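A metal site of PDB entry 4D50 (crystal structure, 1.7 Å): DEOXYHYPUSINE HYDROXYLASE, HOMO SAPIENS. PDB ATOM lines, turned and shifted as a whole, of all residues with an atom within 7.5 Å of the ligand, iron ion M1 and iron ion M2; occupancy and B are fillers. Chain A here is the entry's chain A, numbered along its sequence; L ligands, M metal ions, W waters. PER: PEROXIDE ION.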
ATOM      1  N   LEU A  58     -10.131  14.710  26.501  1.00  0.00           N
ATOM      2  CA  LEU A  58     -11.216  15.676  26.172  1.00  0.00           C
ATOM      3  C   LEU A  58     -12.519  15.279  26.889  1.00  0.00           C
ATOM      4  O   LEU A  58     -13.086  16.080  27.667  1.00  0.00           O
ATOM      5  CB  LEU A  58     -11.494  15.788  24.677  1.00  0.00           C
ATOM      6  CG  LEU A  58     -12.591  16.796  24.375  1.00  0.00           C
ATOM      7  CD1 LEU A  58     -12.144  18.218  24.700  1.00  0.00           C
ATOM      8  CD2 LEU A  58     -13.000  16.784  22.903  1.00  0.00           C
ATOM      9  N   HIS A  61     -12.141  15.423  30.959  1.00  0.00           N
ATOM     10  CA  HIS A  61     -12.097  16.765  31.515  1.00  0.00           C
ATOM     11  C   HIS A  61     -13.468  17.451  31.432  1.00  0.00           C
ATOM     12  O   HIS A  61     -13.837  18.199  32.350  1.00  0.00           O
ATOM     13  CB  HIS A  61     -10.928  17.546  30.929  1.00  0.00           C
ATOM     14  CG  HIS A  61     -11.325  18.606  29.954  1.00  0.00           C
ATOM     15  ND1 HIS A  61     -11.958  18.315  28.765  1.00  0.00           N
ATOM     16  CD2 HIS A  61     -11.226  19.957  30.033  1.00  0.00           C
ATOM     17  CE1 HIS A  61     -12.149  19.462  28.103  1.00  0.00           C
ATOM     18  NE2 HIS A  61     -11.756  20.466  28.882  1.00  0.00           N
ATOM     19  N   GLU A  62     -14.278  17.098  30.432  1.00  0.00           N
ATOM     20  CA  GLU A  62     -15.682  17.624  30.353  1.00  0.00           C
ATOM     21  C   GLU A  62     -16.550  17.011  31.510  1.00  0.00           C
ATOM     22  O   GLU A  62     -17.464  17.645  32.078  1.00  0.00           O
ATOM     23  CB  GLU A  62     -16.266  17.289  29.007  1.00  0.00           C
ATOM     24  CG  GLU A  62     -17.141  18.345  28.359  1.00  0.00           C
ATOM     25  CD  GLU A  62     -16.305  19.499  27.822  1.00  0.00           C
ATOM     26  OE1 GLU A  62     -15.329  19.283  27.074  1.00  0.00           O
ATOM     27  OE2 GLU A  62     -16.572  20.621  28.278  1.00  0.00           O
ATOM     28  N   TYR A  65     -15.689  19.077  34.412  1.00  0.00           N
ATOM     29  CA  TYR A  65     -16.317  20.373  34.288  1.00  0.00           C
ATOM     30  C   TYR A  65     -17.803  20.351  34.641  1.00  0.00           C
ATOM     31  O   TYR A  65     -18.301  21.139  35.429  1.00  0.00           O
ATOM     32  CB  TYR A  65     -16.160  20.897  32.863  1.00  0.00           C
ATOM     33  CG  TYR A  65     -16.861  22.180  32.546  1.00  0.00           C
ATOM     34  CD1 TYR A  65     -16.396  23.398  33.005  1.00  0.00           C
ATOM     35  CD2 TYR A  65     -18.099  22.158  31.889  1.00  0.00           C
ATOM     36  CE1 TYR A  65     -17.070  24.594  32.716  1.00  0.00           C
ATOM     37  CE2 TYR A  65     -18.752  23.320  31.554  1.00  0.00           C
ATOM     38  CZ  TYR A  65     -18.290  24.521  32.042  1.00  0.00           C
ATOM     39  OH  TYR A  65     -18.957  25.630  31.685  1.00  0.00           O
ATOM     40  N   PRO A  90      -2.820  16.468  32.811  1.00  0.00           N
ATOM     41  CA  PRO A  90      -2.936  17.790  33.466  1.00  0.00           C
ATOM     42  C   PRO A  90      -4.311  18.500  33.292  1.00  0.00           C
ATOM     43  O   PRO A  90      -4.869  19.090  34.224  1.00  0.00           O
ATOM     44  CB  PRO A  90      -1.830  18.619  32.783  1.00  0.00           C
ATOM     45  CG  PRO A  90      -0.813  17.623  32.361  1.00  0.00           C
ATOM     46  CD  PRO A  90      -1.558  16.367  32.023  1.00  0.00           C
ATOM     47  N   MET A  91      -4.790  18.475  32.064  1.00  0.00           N
ATOM     48  CA  MET A  91      -6.057  19.087  31.685  1.00  0.00           C
ATOM     49  C   MET A  91      -7.221  18.478  32.498  1.00  0.00           C
ATOM     50  O   MET A  91      -8.183  19.174  32.876  1.00  0.00           O
ATOM     51  CB  MET A  91      -6.217  18.857  30.183  1.00  0.00           C
ATOM     52  CG  MET A  91      -7.562  18.937  29.551  1.00  0.00           C
ATOM     53  SD  MET A  91      -7.230  18.601  27.798  1.00  0.00           S
ATOM     54  CE  MET A  91      -8.855  18.958  27.163  1.00  0.00           C
ATOM     55  N   VAL A  92      -7.110  17.181  32.763  1.00  0.00           N
ATOM     56  CA  VAL A  92      -8.139  16.489  33.457  1.00  0.00           C
ATOM     57  C   VAL A  92      -8.035  16.842  34.973  1.00  0.00           C
ATOM     58  O   VAL A  92      -9.044  17.115  35.635  1.00  0.00           O
ATOM     59  CB  VAL A  92      -8.061  14.974  33.218  1.00  0.00           C
ATOM     60  CG1 VAL A  92      -9.010  14.279  34.108  1.00  0.00           C
ATOM     61  CG2 VAL A  92      -8.455  14.671  31.755  1.00  0.00           C
ATOM     62  N   HIS A  94      -6.563  19.430  36.302  1.00  0.00           N
ATOM     63  CA  HIS A  94      -6.897  20.866  36.458  1.00  0.00           C
ATOM     64  C   HIS A  94      -8.401  20.987  36.553  1.00  0.00           C
ATOM     65  O   HIS A  94      -8.950  21.660  37.507  1.00  0.00           O
ATOM     66  CB  HIS A  94      -6.328  21.755  35.321  1.00  0.00           C
ATOM     67  CG  HIS A  94      -7.358  22.611  34.692  1.00  0.00           C
ATOM     68  ND1 HIS A  94      -7.897  23.727  35.296  1.00  0.00           N
ATOM     69  CD2 HIS A  94      -7.962  22.490  33.489  1.00  0.00           C
ATOM     70  CE1 HIS A  94      -8.815  24.236  34.498  1.00  0.00           C
ATOM     71  NE2 HIS A  94      -8.864  23.503  33.396  1.00  0.00           N
ATOM     72  N   GLU A  95      -9.106  20.350  35.642  1.00  0.00           N
ATOM     73  CA  GLU A  95     -10.546  20.498  35.573  1.00  0.00           C
ATOM     74  C   GLU A  95     -11.230  20.016  36.864  1.00  0.00           C
ATOM     75  O   GLU A  95     -12.217  20.565  37.318  1.00  0.00           O
ATOM     76  CB  GLU A  95     -11.186  19.840  34.323  1.00  0.00           C
ATOM     77  CG  GLU A  95     -12.420  20.528  33.838  1.00  0.00           C
ATOM     78  CD  GLU A  95     -12.167  21.927  33.312  1.00  0.00           C
ATOM     79  OE1 GLU A  95     -11.241  22.164  32.442  1.00  0.00           O
ATOM     80  OE2 GLU A  95     -12.822  22.884  33.821  1.00  0.00           O
ATOM     81  N   GLU A  98     -10.558  22.733  39.599  1.00  0.00           N
ATOM     82  CA  GLU A  98     -11.545  23.804  39.356  1.00  0.00           C
ATOM     83  C   GLU A  98     -12.982  23.436  39.775  1.00  0.00           C
ATOM     84  O   GLU A  98     -13.684  24.245  40.329  1.00  0.00           O
ATOM     85  CB  GLU A  98     -11.561  24.262  37.865  1.00  0.00           C
ATOM     86  CG  GLU A  98     -12.530  25.423  37.624  1.00  0.00           C
ATOM     87  CD  GLU A  98     -12.503  25.988  36.221  1.00  0.00           C
ATOM     88  OE1 GLU A  98     -11.406  26.061  35.627  1.00  0.00           O
ATOM     89  OE2 GLU A  98     -13.575  26.443  35.788  1.00  0.00           O
ATOM     90  N   THR A 126      -4.607  26.194  39.091  1.00  0.00           N
ATOM     91  CA  THR A 126      -6.057  25.964  39.231  1.00  0.00           C
ATOM     92  C   THR A 126      -6.436  25.936  40.735  1.00  0.00           C
ATOM     93  O   THR A 126      -7.424  26.564  41.116  1.00  0.00           O
ATOM     94  CB  THR A 126      -6.444  24.591  38.681  1.00  0.00           C
ATOM     95  OG1 THR A 126      -6.217  24.643  37.251  1.00  0.00           O
ATOM     96  CG2 THR A 126      -7.837  24.218  39.004  1.00  0.00           C
ATOM     97  N   LEU A 209      -2.723  27.835  31.534  1.00  0.00           N
ATOM     98  CA  LEU A 209      -4.061  27.897  32.180  1.00  0.00           C
ATOM     99  C   LEU A 209      -4.762  29.190  31.840  1.00  0.00           C
ATOM    100  O   LEU A 209      -5.920  29.195  31.365  1.00  0.00           O
ATOM    101  CB  LEU A 209      -3.947  27.759  33.696  1.00  0.00           C
ATOM    102  CG  LEU A 209      -5.236  27.343  34.365  1.00  0.00           C
ATOM    103  CD1 LEU A 209      -5.598  25.916  34.102  1.00  0.00           C
ATOM    104  CD2 LEU A 209      -5.173  27.611  35.855  1.00  0.00           C
ATOM    105  N   HIS A 212      -5.887  29.429  28.186  1.00  0.00           N
ATOM    106  CA  HIS A 212      -7.018  28.565  27.938  1.00  0.00           C
ATOM    107  C   HIS A 212      -8.291  29.194  28.417  1.00  0.00           C
ATOM    108  O   HIS A 212      -9.324  29.081  27.773  1.00  0.00           O
ATOM    109  CB  HIS A 212      -6.718  27.132  28.471  1.00  0.00           C
ATOM    110  CG  HIS A 212      -7.596  26.601  29.552  1.00  0.00           C
ATOM    111  ND1 HIS A 212      -7.500  27.020  30.856  1.00  0.00           N
ATOM    112  CD2 HIS A 212      -8.443  25.543  29.576  1.00  0.00           C
ATOM    113  CE1 HIS A 212      -8.386  26.395  31.583  1.00  0.00           C
ATOM    114  NE2 HIS A 212      -8.936  25.455  30.854  1.00  0.00           N
ATOM    115  N   GLU A 213      -8.230  29.803  29.595  1.00  0.00           N
ATOM    116  CA  GLU A 213      -9.370  30.508  30.111  1.00  0.00           C
ATOM    117  C   GLU A 213      -9.823  31.615  29.192  1.00  0.00           C
ATOM    118  O   GLU A 213     -11.038  31.830  29.021  1.00  0.00           O
ATOM    119  CB  GLU A 213      -9.093  31.015  31.531  1.00  0.00           C
ATOM    120  CG  GLU A 213     -10.357  31.337  32.266  1.00  0.00           C
ATOM    121  CD  GLU A 213     -11.199  30.114  32.633  1.00  0.00           C
ATOM    122  OE1 GLU A 213     -10.639  29.070  33.020  1.00  0.00           O
ATOM    123  OE2 GLU A 213     -12.450  30.248  32.543  1.00  0.00           O
ATOM    124  N   TYR A 216     -11.824  30.056  26.550  1.00  0.00           N
ATOM    125  CA  TYR A 216     -13.159  29.709  27.023  1.00  0.00           C
ATOM    126  C   TYR A 216     -14.083  30.951  27.058  1.00  0.00           C
ATOM    127  O   TYR A 216     -15.202  30.927  26.521  1.00  0.00           O
ATOM    128  CB  TYR A 216     -13.031  29.027  28.411  1.00  0.00           C
ATOM    129  CG  TYR A 216     -14.320  28.816  29.192  1.00  0.00           C
ATOM    130  CD1 TYR A 216     -14.802  29.792  30.099  1.00  0.00           C
ATOM    131  CD2 TYR A 216     -15.040  27.612  29.084  1.00  0.00           C
ATOM    132  CE1 TYR A 216     -16.000  29.584  30.839  1.00  0.00           C
ATOM    133  CE2 TYR A 216     -16.198  27.405  29.832  1.00  0.00           C
ATOM    134  CZ  TYR A 216     -16.682  28.409  30.671  1.00  0.00           C
ATOM    135  OH  TYR A 216     -17.833  28.153  31.464  1.00  0.00           O
ATOM    136  N   ASN A 240       0.217  25.215  23.532  1.00  0.00           N
ATOM    137  CA  ASN A 240      -0.191  24.119  24.382  1.00  0.00           C
ATOM    138  C   ASN A 240      -1.518  23.483  23.903  1.00  0.00           C
ATOM    139  O   ASN A 240      -2.418  24.207  23.528  1.00  0.00           O
ATOM    140  CB  ASN A 240      -0.312  24.714  25.785  1.00  0.00           C
ATOM    141  CG  ASN A 240      -0.712  23.703  26.776  1.00  0.00           C
ATOM    142  OD1 ASN A 240      -1.812  23.242  26.781  1.00  0.00           O
ATOM    143  ND2 ASN A 240       0.204  23.320  27.622  1.00  0.00           N
ATOM    144  N   PRO A 241      -1.600  22.138  23.808  1.00  0.00           N
ATOM    145  CA  PRO A 241      -2.767  21.473  23.289  1.00  0.00           C
ATOM    146  C   PRO A 241      -4.053  21.809  24.062  1.00  0.00           C
ATOM    147  O   PRO A 241      -5.145  21.947  23.451  1.00  0.00           O
ATOM    148  CB  PRO A 241      -2.461  19.978  23.415  1.00  0.00           C
ATOM    149  CG  PRO A 241      -1.043  19.894  23.817  1.00  0.00           C
ATOM    150  CD  PRO A 241      -0.441  21.228  23.962  1.00  0.00           C
ATOM    151  N   MET A 242      -3.943  22.060  25.358  1.00  0.00           N
ATOM    152  CA  MET A 242      -5.106  22.467  26.156  1.00  0.00           C
ATOM    153  C   MET A 242      -5.631  23.842  25.704  1.00  0.00           C
ATOM    154  O   MET A 242      -6.844  24.072  25.684  1.00  0.00           O
ATOM    155  CB  MET A 242      -4.696  22.500  27.638  1.00  0.00           C
ATOM    156  CG  MET A 242      -5.725  23.036  28.589  1.00  0.00           C
ATOM    157  SD  MET A 242      -5.134  23.017  30.287  1.00  0.00           S
ATOM    158  CE  MET A 242      -4.180  24.537  30.162  1.00  0.00           C
ATOM    159  N   VAL A 243      -4.736  24.760  25.353  1.00  0.00           N
ATOM    160  CA  VAL A 243      -5.114  26.083  24.824  1.00  0.00           C
ATOM    161  C   VAL A 243      -5.700  25.952  23.387  1.00  0.00           C
ATOM    162  O   VAL A 243      -6.758  26.554  23.054  1.00  0.00           O
ATOM    163  CB  VAL A 243      -3.917  27.043  24.708  1.00  0.00           C
ATOM    164  CG1 VAL A 243      -4.334  28.344  24.096  1.00  0.00           C
ATOM    165  CG2 VAL A 243      -3.294  27.284  26.133  1.00  0.00           C
ATOM    166  N   HIS A 245      -7.114  23.347  22.070  1.00  0.00           N
ATOM    167  CA  HIS A 245      -8.480  22.746  22.251  1.00  0.00           C
ATOM    168  C   HIS A 245      -9.543  23.758  22.664  1.00  0.00           C
ATOM    169  O   HIS A 245     -10.662  23.764  22.113  1.00  0.00           O
ATOM    170  CB  HIS A 245      -8.465  21.564  23.201  1.00  0.00           C
ATOM    171  CG  HIS A 245      -9.483  21.662  24.268  1.00  0.00           C
ATOM    172  ND1 HIS A 245     -10.806  21.339  24.037  1.00  0.00           N
ATOM    173  CD2 HIS A 245      -9.395  21.957  25.587  1.00  0.00           C
ATOM    174  CE1 HIS A 245     -11.492  21.537  25.141  1.00  0.00           C
ATOM    175  NE2 HIS A 245     -10.653  21.830  26.119  1.00  0.00           N
ATOM    176  N   GLU A 246      -9.219  24.670  23.610  1.00  0.00           N
ATOM    177  CA  GLU A 246     -10.187  25.610  24.079  1.00  0.00           C
ATOM    178  C   GLU A 246     -10.571  26.616  22.977  1.00  0.00           C
ATOM    179  O   GLU A 246     -11.743  26.971  22.850  1.00  0.00           O
ATOM    180  CB  GLU A 246      -9.645  26.311  25.355  1.00  0.00           C
ATOM    181  CG  GLU A 246     -10.718  26.655  26.350  1.00  0.00           C
ATOM    182  CD  GLU A 246     -11.433  25.446  26.878  1.00  0.00           C
ATOM    183  OE1 GLU A 246     -10.810  24.541  27.438  1.00  0.00           O
ATOM    184  OE2 GLU A 246     -12.667  25.415  26.683  1.00  0.00           O
ATOM    185  N   GLU A 249     -12.905  24.834  20.589  1.00  0.00           N
ATOM    186  CA  GLU A 249     -14.238  24.858  21.174  1.00  0.00           C
ATOM    187  C   GLU A 249     -14.890  26.199  20.990  1.00  0.00           C
ATOM    188  O   GLU A 249     -16.061  26.256  20.670  1.00  0.00           O
ATOM    189  CB  GLU A 249     -14.220  24.529  22.670  1.00  0.00           C
ATOM    190  CG  GLU A 249     -14.241  23.072  23.031  1.00  0.00           C
ATOM    191  CD  GLU A 249     -15.044  22.766  24.329  1.00  0.00           C
ATOM    192  OE1 GLU A 249     -15.805  23.576  24.899  1.00  0.00           O
ATOM    193  OE2 GLU A 249     -14.890  21.639  24.774  1.00  0.00           O
ATOM    194  N   VAL A 273      -6.510  15.702  21.580  1.00  0.00           N
ATOM    195  CA  VAL A 273      -7.447  16.613  22.217  1.00  0.00           C
ATOM    196  C   VAL A 273      -7.946  17.694  21.204  1.00  0.00           C
ATOM    197  O   VAL A 273      -9.128  18.090  21.188  1.00  0.00           O
ATOM    198  CB  VAL A 273      -6.852  17.264  23.466  1.00  0.00           C
ATOM    199  CG1 VAL A 273      -7.933  18.000  24.224  1.00  0.00           C
ATOM    200  CG2 VAL A 273      -6.201  16.219  24.378  1.00  0.00           C
ATOM    201  N   SER A 277     -11.803  17.920  19.668  1.00  0.00           N
ATOM    202  CA  SER A 277     -12.553  19.191  19.777  1.00  0.00           C
ATOM    203  C   SER A 277     -13.102  19.635  18.435  1.00  0.00           C
ATOM    204  O   SER A 277     -14.276  20.052  18.347  1.00  0.00           O
ATOM    205  CB  SER A 277     -11.788  20.363  20.429  1.00  0.00           C
ATOM    206  OG  SER A 277     -11.619  20.030  21.777  1.00  0.00           O
HETATM  207  O1  PER L   1      -9.209  22.354  30.116  1.00  0.00           O
HETATM  208  O2  PER L   1      -8.995  22.426  28.583  1.00  0.00           O
HETATM  209 FE    FE M   1     -11.125  22.588  28.131  1.00  0.00          FE
HETATM  210 FE    FE M   2     -10.169  23.706  31.591  1.00  0.00          FE
HETATM  211  O   HOH W   1     -13.194  22.921  27.602  1.00  0.00           O
HETATM  212  O   HOH W   2     -11.403  25.157  32.652  1.00  0.00           O
HETATM  213  O   HOH W   3     -11.731  23.730  30.122  1.00  0.00           O
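A ring nitrogen (ND1) of His 245 is in hydrogen-bond range of the side-chain hydroxyl (OG) of Ser 277 (2.7 Å). A ring nitrogen (ND1) of His 94 sits at hydrogen-bond distance from the side-chain hydroxyl (OG1) of Thr 126, at 2.7 Å. The backbone carbonyl oxygen (O) of Leu 209 sits at hydrogen-bond distance from a ring nitrogen (ND1) of His 212, at 2.7 Å. ND1 of His 61 sits at hydrogen-bond distance from O of Leu 58, 2.7 Å away. N of Met 242 lies within hydrogen-bond range of OD1 of Asn 240 (2.8 Å).
Residues that only touch the ligand: Met 242 and Met 91. Eight residues have an atom within 4 Å of the ligand: His 61, Met 91, His 94, Glu 95, His 212, Met 242, His 245 and Glu 246.
Within 4 Å of iron ion M1: His 61, His 245 and Glu 246. The nearest printed residue that does not touch iron ion M1 is His 212 (4.2 Å).
Within 4 Å of iron ion M2: His 94, Glu 95 and His 212.
OE1 of Glu 246 is bound to iron ion M1. Water W1 binds iron ion M1 (2.2 Å). Iron ion M1 is bound by O2 of the ligand (2.2 Å). Iron ion M1 is bound by NE2 of His 245. A ring nitrogen (NE2) of His 61 binds iron ion M1 (2.3 Å). Iron ion M1 is bound by water W3. Iron ion M1 has six donor atoms within binding distance.
Iron ion M2 is bound by the side-chain carboxylate (OE1) of Glu 95 (2.1 Å). Water W3 binds iron ion M2, at 2.1 Å. Water W2 binds iron ion M2, 2.2 Å away. An oxygen (O1) of the ligand is bound to iron ion M2, at 2.2 Å. NE2 of His 94 binds iron ion M2 (2.2 Å). NE2 of His 212 binds iron ion M2, at 2.3 Å. Iron ion M2 has six donor atoms within binding distance.
Water W2 lies within hydrogen-bond range of the side-chain carboxylate (OE2) of Glu 95 (2.9 Å) and the side-chain carboxylate (OE1) of Glu 98 (3.1 Å).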
